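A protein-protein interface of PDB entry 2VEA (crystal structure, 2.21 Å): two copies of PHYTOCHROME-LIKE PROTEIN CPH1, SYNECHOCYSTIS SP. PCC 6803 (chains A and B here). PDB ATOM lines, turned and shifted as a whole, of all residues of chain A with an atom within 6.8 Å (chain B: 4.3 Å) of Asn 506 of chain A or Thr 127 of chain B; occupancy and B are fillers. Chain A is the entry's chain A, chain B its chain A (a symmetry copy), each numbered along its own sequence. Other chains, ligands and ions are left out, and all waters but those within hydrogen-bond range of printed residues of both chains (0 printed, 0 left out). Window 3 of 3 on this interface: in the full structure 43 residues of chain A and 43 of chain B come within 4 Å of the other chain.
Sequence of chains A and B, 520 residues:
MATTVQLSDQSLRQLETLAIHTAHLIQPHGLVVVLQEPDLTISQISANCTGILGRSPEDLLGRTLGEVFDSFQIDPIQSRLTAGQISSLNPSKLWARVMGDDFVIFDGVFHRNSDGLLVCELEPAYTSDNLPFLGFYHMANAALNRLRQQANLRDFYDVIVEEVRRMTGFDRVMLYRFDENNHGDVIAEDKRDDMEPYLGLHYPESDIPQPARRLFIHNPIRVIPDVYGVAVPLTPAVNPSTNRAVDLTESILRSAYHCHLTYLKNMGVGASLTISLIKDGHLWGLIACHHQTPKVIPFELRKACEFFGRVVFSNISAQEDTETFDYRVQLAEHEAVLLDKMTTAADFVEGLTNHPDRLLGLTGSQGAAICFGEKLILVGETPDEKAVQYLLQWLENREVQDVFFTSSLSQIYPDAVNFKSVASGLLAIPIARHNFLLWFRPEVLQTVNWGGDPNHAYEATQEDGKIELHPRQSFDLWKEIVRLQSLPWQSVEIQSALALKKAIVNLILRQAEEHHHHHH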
ATOM      1  N   LEU A 500      22.382  -4.936  -2.990  1.00  0.00           N
ATOM      2  CA  LEU A 500      23.325  -6.034  -2.773  1.00  0.00           C
ATOM      3  C   LEU A 500      23.117  -7.115  -3.837  1.00  0.00           C
ATOM      4  O   LEU A 500      24.083  -7.580  -4.455  1.00  0.00           O
ATOM      5  CB  LEU A 500      23.151  -6.626  -1.367  1.00  0.00           C
ATOM      6  CG  LEU A 500      24.367  -7.286  -0.696  1.00  0.00           C
ATOM      7  CD1 LEU A 500      23.920  -8.130   0.496  1.00  0.00           C
ATOM      8  CD2 LEU A 500      25.171  -8.135  -1.668  1.00  0.00           C
ATOM      9  N   LYS A 501      21.859  -7.507  -4.047  1.00  0.00           N
ATOM     10  CA  LYS A 501      21.504  -8.489  -5.078  1.00  0.00           C
ATOM     11  C   LYS A 501      22.035  -8.077  -6.448  1.00  0.00           C
ATOM     12  O   LYS A 501      22.516  -8.917  -7.210  1.00  0.00           O
ATOM     13  CB  LYS A 501      19.984  -8.661  -5.170  1.00  0.00           C
ATOM     14  CG  LYS A 501      19.533  -9.719  -6.197  1.00  0.00           C
ATOM     15  CD  LYS A 501      18.332  -9.267  -7.039  1.00  0.00           C
ATOM     16  CE  LYS A 501      18.407  -9.807  -8.477  1.00  0.00           C
ATOM     17  NZ  LYS A 501      18.700 -11.267  -8.559  1.00  0.00           N
ATOM     18  N   LYS A 502      21.931  -6.787  -6.754  1.00  0.00           N
ATOM     19  CA  LYS A 502      22.390  -6.258  -8.032  1.00  0.00           C
ATOM     20  C   LYS A 502      23.912  -6.258  -8.128  1.00  0.00           C
ATOM     21  O   LYS A 502      24.459  -6.494  -9.200  1.00  0.00           O
ATOM     22  CB  LYS A 502      21.825  -4.856  -8.265  1.00  0.00           C
ATOM     23  CG  LYS A 502      20.325  -4.866  -8.564  1.00  0.00           C
ATOM     24  CD  LYS A 502      19.770  -3.473  -8.833  1.00  0.00           C
ATOM     25  CE  LYS A 502      18.321  -3.531  -9.311  1.00  0.00           C
ATOM     26  NZ  LYS A 502      17.340  -3.733  -8.205  1.00  0.00           N
ATOM     27  N   ALA A 503      24.584  -6.000  -7.007  1.00  0.00           N
ATOM     28  CA  ALA A 503      26.049  -6.060  -6.943  1.00  0.00           C
ATOM     29  C   ALA A 503      26.556  -7.491  -7.066  1.00  0.00           C
ATOM     30  O   ALA A 503      27.624  -7.724  -7.628  1.00  0.00           O
ATOM     31  CB  ALA A 503      26.553  -5.443  -5.651  1.00  0.00           C
ATOM     32  N   ILE A 504      25.796  -8.445  -6.530  1.00  0.00           N
ATOM     33  CA  ILE A 504      26.137  -9.862  -6.668  1.00  0.00           C
ATOM     34  C   ILE A 504      25.965 -10.300  -8.119  1.00  0.00           C
ATOM     35  O   ILE A 504      26.832 -10.968  -8.675  1.00  0.00           O
ATOM     36  CB  ILE A 504      25.286 -10.749  -5.731  1.00  0.00           C
ATOM     37  CG1 ILE A 504      25.712 -10.531  -4.278  1.00  0.00           C
ATOM     38  CG2 ILE A 504      25.441 -12.225  -6.089  1.00  0.00           C
ATOM     39  CD1 ILE A 504      24.776 -11.137  -3.273  1.00  0.00           C
ATOM     40  N   VAL A 505      24.852  -9.906  -8.726  1.00  0.00           N
ATOM     41  CA  VAL A 505      24.587 -10.176 -10.141  1.00  0.00           C
ATOM     42  C   VAL A 505      25.664  -9.549 -11.035  1.00  0.00           C
ATOM     43  O   VAL A 505      26.019 -10.111 -12.070  1.00  0.00           O
ATOM     44  CB  VAL A 505      23.178  -9.656 -10.552  1.00  0.00           C
ATOM     45  CG1 VAL A 505      22.988  -9.704 -12.066  1.00  0.00           C
ATOM     46  CG2 VAL A 505      22.087 -10.457  -9.847  1.00  0.00           C
ATOM     47  N   ASN A 506      26.174  -8.389 -10.625  1.00  0.00           N
ATOM     48  CA  ASN A 506      27.286  -7.735 -11.315  1.00  0.00           C
ATOM     49  C   ASN A 506      28.519  -8.623 -11.355  1.00  0.00           C
ATOM     50  O   ASN A 506      29.215  -8.671 -12.366  1.00  0.00           O
ATOM     51  CB  ASN A 506      27.658  -6.406 -10.641  1.00  0.00           C
ATOM     52  CG  ASN A 506      26.834  -5.231 -11.137  1.00  0.00           C
ATOM     53  OD1 ASN A 506      25.781  -5.400 -11.751  1.00  0.00           O
ATOM     54  ND2 ASN A 506      27.312  -4.026 -10.860  1.00  0.00           N
ATOM     55  N   LEU A 507      28.783  -9.315 -10.249  1.00  0.00           N
ATOM     56  CA  LEU A 507      29.959 -10.177 -10.137  1.00  0.00           C
ATOM     57  C   LEU A 507      29.842 -11.447 -10.971  1.00  0.00           C
ATOM     58  O   LEU A 507      30.806 -11.832 -11.627  1.00  0.00           O
ATOM     59  CB  LEU A 507      30.237 -10.523  -8.674  1.00  0.00           C
ATOM     60  CG  LEU A 507      30.700  -9.330  -7.843  1.00  0.00           C
ATOM     61  CD1 LEU A 507      30.767  -9.681  -6.370  1.00  0.00           C
ATOM     62  CD2 LEU A 507      32.056  -8.847  -8.347  1.00  0.00           C
ATOM     63  N   ILE A 508      28.677 -12.093 -10.952  1.00  0.00           N
ATOM     64  CA  ILE A 508      28.432 -13.247 -11.827  1.00  0.00           C
ATOM     65  C   ILE A 508      28.606 -12.843 -13.294  1.00  0.00           C
ATOM     66  O   ILE A 508      29.232 -13.568 -14.075  1.00  0.00           O
ATOM     67  CB  ILE A 508      27.015 -13.864 -11.632  1.00  0.00           C
ATOM     68  CG1 ILE A 508      26.914 -14.629 -10.304  1.00  0.00           C
ATOM     69  CG2 ILE A 508      26.676 -14.816 -12.776  1.00  0.00           C
ATOM     70  CD1 ILE A 508      26.364 -13.813  -9.161  1.00  0.00           C
ATOM     71  N   LEU A 509      28.058 -11.683 -13.657  1.00  0.00           N
ATOM     72  CA  LEU A 509      28.228 -11.130 -15.006  1.00  0.00           C
ATOM     73  C   LEU A 509      29.686 -10.778 -15.322  1.00  0.00           C
ATOM     74  O   LEU A 509      30.134 -10.964 -16.456  1.00  0.00           O
ATOM     75  CB  LEU A 509      27.337  -9.895 -15.211  1.00  0.00           C
ATOM     76  CG  LEU A 509      25.902 -10.141 -15.695  1.00  0.00           C
ATOM     77  CD1 LEU A 509      25.899 -10.672 -17.124  1.00  0.00           C
ATOM     78  CD2 LEU A 509      25.172 -11.090 -14.769  1.00  0.00           C
ATOM     79  N   ARG A 510      30.422 -10.272 -14.334  1.00  0.00           N
ATOM     80  CA  ARG A 510      31.844  -9.956 -14.526  1.00  0.00           C
ATOM     81  C   ARG A 510      32.631 -11.228 -14.849  1.00  0.00           C
ATOM     82  O   ARG A 510      33.427 -11.240 -15.785  1.00  0.00           O
ATOM     83  CB  ARG A 510      32.435  -9.259 -13.295  1.00  0.00           C
ATOM     84  CG  ARG A 510      33.706  -8.480 -13.578  1.00  0.00           C
ATOM     85  N   GLN A 511      32.388 -12.291 -14.079  1.00  0.00           N
ATOM     86  CA  GLN A 511      32.955 -13.616 -14.360  1.00  0.00           C
ATOM     87  C   GLN A 511      32.572 -14.104 -15.752  1.00  0.00           C
ATOM     88  O   GLN A 511      33.433 -14.517 -16.532  1.00  0.00           O
ATOM     89  CB  GLN A 511      32.456 -14.654 -13.350  1.00  0.00           C
ATOM     90  CG  GLN A 511      32.965 -14.493 -11.929  1.00  0.00           C
ATOM     91  CD  GLN A 511      32.508 -15.634 -11.022  1.00  0.00           C
ATOM     92  OE1 GLN A 511      32.938 -16.784 -11.184  1.00  0.00           O
ATOM     93  NE2 GLN A 511      31.635 -15.318 -10.059  1.00  0.00           N
ATOM     94  N   GLU A 513      31.725 -12.681 -18.532  1.00  0.00           N
ATOM     95  CA  GLU A 513      32.434 -12.030 -19.637  1.00  0.00           C
ATOM     96  C   GLU A 513      33.957 -12.132 -19.509  1.00  0.00           C
ATOM     97  O   GLU A 513      34.674 -11.909 -20.485  1.00  0.00           O
ATOM     98  CB  GLU A 513      31.989 -10.567 -19.796  1.00  0.00           C
ATOM     99  CG  GLU A 513      32.567  -9.571 -18.801  1.00  0.00           C
ATOM    100  CD  GLU A 513      31.938  -8.191 -18.949  1.00  0.00           C
ATOM    101  OE1 GLU A 513      32.618  -7.276 -19.466  1.00  0.00           O
ATOM    102  OE2 GLU A 513      30.760  -8.027 -18.563  1.00  0.00           O
ATOM    103  N   LYS B  93      19.542  -6.293 -15.402  1.00  0.00           N
ATOM    104  CA  LYS B  93      20.550  -6.720 -16.366  1.00  0.00           C
ATOM    105  C   LYS B  93      19.925  -7.576 -17.458  1.00  0.00           C
ATOM    106  O   LYS B  93      19.341  -8.626 -17.176  1.00  0.00           O
ATOM    107  CB  LYS B  93      21.663  -7.517 -15.685  1.00  0.00           C
ATOM    108  CG  LYS B  93      22.566  -6.698 -14.780  1.00  0.00           C
ATOM    109  CD  LYS B  93      23.566  -5.869 -15.583  1.00  0.00           C
ATOM    110  CE  LYS B  93      24.496  -5.094 -14.676  1.00  0.00           C
ATOM    111  NZ  LYS B  93      23.741  -4.152 -13.803  1.00  0.00           N
ATOM    112  N   ASP B 107      21.759  -2.598 -19.094  1.00  0.00           N
ATOM    113  CA  ASP B 107      20.907  -2.310 -17.949  1.00  0.00           C
ATOM    114  C   ASP B 107      19.625  -1.710 -18.495  1.00  0.00           C
ATOM    115  O   ASP B 107      19.622  -0.583 -18.977  1.00  0.00           O
ATOM    116  CB  ASP B 107      21.578  -1.327 -16.986  1.00  0.00           C
ATOM    117  CG  ASP B 107      22.323  -2.027 -15.875  1.00  0.00           C
ATOM    118  OD1 ASP B 107      23.513  -1.706 -15.661  1.00  0.00           O
ATOM    119  OD2 ASP B 107      21.722  -2.911 -15.222  1.00  0.00           O
ATOM    120  N   ALA B 125      25.618  -1.489 -20.151  1.00  0.00           N
ATOM    121  CA  ALA B 125      26.084  -1.530 -18.765  1.00  0.00           C
ATOM    122  C   ALA B 125      27.601  -1.634 -18.723  1.00  0.00           C
ATOM    123  O   ALA B 125      28.182  -2.527 -19.330  1.00  0.00           O
ATOM    124  CB  ALA B 125      25.455  -2.705 -18.031  1.00  0.00           C
ATOM    125  N   TYR B 126      28.238  -0.695 -18.029  1.00  0.00           N
ATOM    126  CA  TYR B 126      29.682  -0.736 -17.794  1.00  0.00           C
ATOM    127  C   TYR B 126      29.981  -1.266 -16.399  1.00  0.00           C
ATOM    128  O   TYR B 126      31.014  -1.901 -16.176  1.00  0.00           O
ATOM    129  CB  TYR B 126      30.288   0.658 -17.947  1.00  0.00           C
ATOM    130  CG  TYR B 126      29.997   1.291 -19.282  1.00  0.00           C
ATOM    131  CD1 TYR B 126      30.780   1.003 -20.394  1.00  0.00           C
ATOM    132  CD2 TYR B 126      28.932   2.170 -19.437  1.00  0.00           C
ATOM    133  CE1 TYR B 126      30.513   1.579 -21.629  1.00  0.00           C
ATOM    134  CE2 TYR B 126      28.654   2.752 -20.665  1.00  0.00           C
ATOM    135  CZ  TYR B 126      29.449   2.453 -21.758  1.00  0.00           C
ATOM    136  OH  TYR B 126      29.177   3.028 -22.977  1.00  0.00           O
ATOM    137  N   THR B 127      29.070  -1.005 -15.467  1.00  0.00           N
ATOM    138  CA  THR B 127      29.291  -1.308 -14.063  1.00  0.00           C
ATOM    139  C   THR B 127      29.100  -2.789 -13.746  1.00  0.00           C
ATOM    140  O   THR B 127      28.061  -3.199 -13.230  1.00  0.00           O
ATOM    141  CB  THR B 127      28.363  -0.465 -13.163  1.00  0.00           C
ATOM    142  OG1 THR B 127      26.993  -0.708 -13.510  1.00  0.00           O
ATOM    143  CG2 THR B 127      28.668   1.022 -13.320  1.00  0.00           C
ATOM    144  N   SER B 128      30.106  -3.586 -14.092  1.00  0.00           N
ATOM    145  CA  SER B 128      30.295  -4.902 -13.493  1.00  0.00           C
ATOM    146  C   SER B 128      31.092  -4.699 -12.199  1.00  0.00           C
ATOM    147  O   SER B 128      30.993  -5.495 -11.262  1.00  0.00           O
ATOM    148  CB  SER B 128      31.039  -5.832 -14.449  1.00  0.00           C
ATOM    149  OG  SER B 128      30.340  -5.963 -15.675  1.00  0.00           O
ATOM    150  N   ASP B 129      31.886  -3.624 -12.176  1.00  0.00           N
ATOM    151  CA  ASP B 129      32.568  -3.136 -10.971  1.00  0.00           C
ATOM    152  C   ASP B 129      32.190  -1.668 -10.761  1.00  0.00           C
ATOM    153  O   ASP B 129      32.229  -0.867 -11.697  1.00  0.00           O
ATOM    154  CB  ASP B 129      34.088  -3.309 -11.082  1.00  0.00           C
ATOM    155  CG  ASP B 129      34.598  -3.127 -12.497  1.00  0.00           C
ATOM    156  OD1 ASP B 129      35.532  -3.859 -12.884  1.00  0.00           O
ATOM    157  OD2 ASP B 129      34.054  -2.270 -13.225  1.00  0.00           O
ATOM    158  N   ASN B 130      31.846  -1.325  -9.522  1.00  0.00           N
ATOM    159  CA  ASN B 130      31.045  -0.135  -9.230  1.00  0.00           C
ATOM    160  C   ASN B 130      31.629   0.841  -8.207  1.00  0.00           C
ATOM    161  O   ASN B 130      32.522   0.497  -7.433  1.00  0.00           O
ATOM    162  CB  ASN B 130      29.670  -0.593  -8.711  1.00  0.00           C
ATOM    163  CG  ASN B 130      28.519  -0.199  -9.629  1.00  0.00           C
ATOM    164  OD1 ASN B 130      28.527   0.873 -10.237  1.00  0.00           O
ATOM    165  ND2 ASN B 130      27.507  -1.059  -9.709  1.00  0.00           N
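The side-chain carboxylate (OD2) of Asp 107 of chain B is in salt-bridge range of the side-chain amino group (NZ) of Lys 93 of chain B, 2.8 Å away.
The side-chain amide oxygen (OD1) of Asn 506 of chain A sits close to the backbone carbonyl oxygen (O) of Lys 502 of chain A, at 3.1 Å.
The side-chain amide oxygen of Asn 506 of chain A is in hydrogen-bond range of the side-chain amino group of Lys 93 of chain B.
ND2 of Asn 506 of chain A is in hydrogen-bond range of O of Thr 127 of chain B.
ND2 of Asn 506 of chain A lies close to ND2 of Asn 130 of chain B (3.2 Å).
Thr 127 of chain B touches one residue of chain A.
Printed residues of chain B within 4 Å of Arg 510 of chain A: Ser 128.
Of the printed residues of chain A, Ser 128 of chain B touches Asn 506 (3.5 Å), Arg 510 (3.9 Å) and Glu 513 (3.6 Å).
Of the printed residues of chain A, Asn 130 of chain B touches Asn 506.
Of the printed residues of chain A, Lys 93 of chain B touches Asn 506.
Lys 502 of chain A touches none of the printed residues of chain B.
The nearest printed residue of chain B that does not touch Asn 506 of chain A is Asp 129 of chain B (4.8 Å).
The nearest residue of chain A that does not touch Thr 127 of chain B is Lys 502 of chain A (6.3 Å).
Asn 506 of chain A touches Ser 128 of chain B.
Ser 128 of chain B touches Arg 510 of chain A (CB to CG, 3.9 Å).
OE2 of Glu 513 of chain A touches OG of Ser 128 of chain B, 3.6 Å away.
Along chain B the printed residues that touch a printed residue of chain A span positions 93 to 130.
Of the 13 printed residues of chain A, 3 touch a printed residue of chain B.
Among the printed residues, 6 pairs touch across the chains.
No position is printed for both chains.
Of the 6 pairs that touch across the chains among the printed residues, none has its exchanged pair printed and touching as well.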
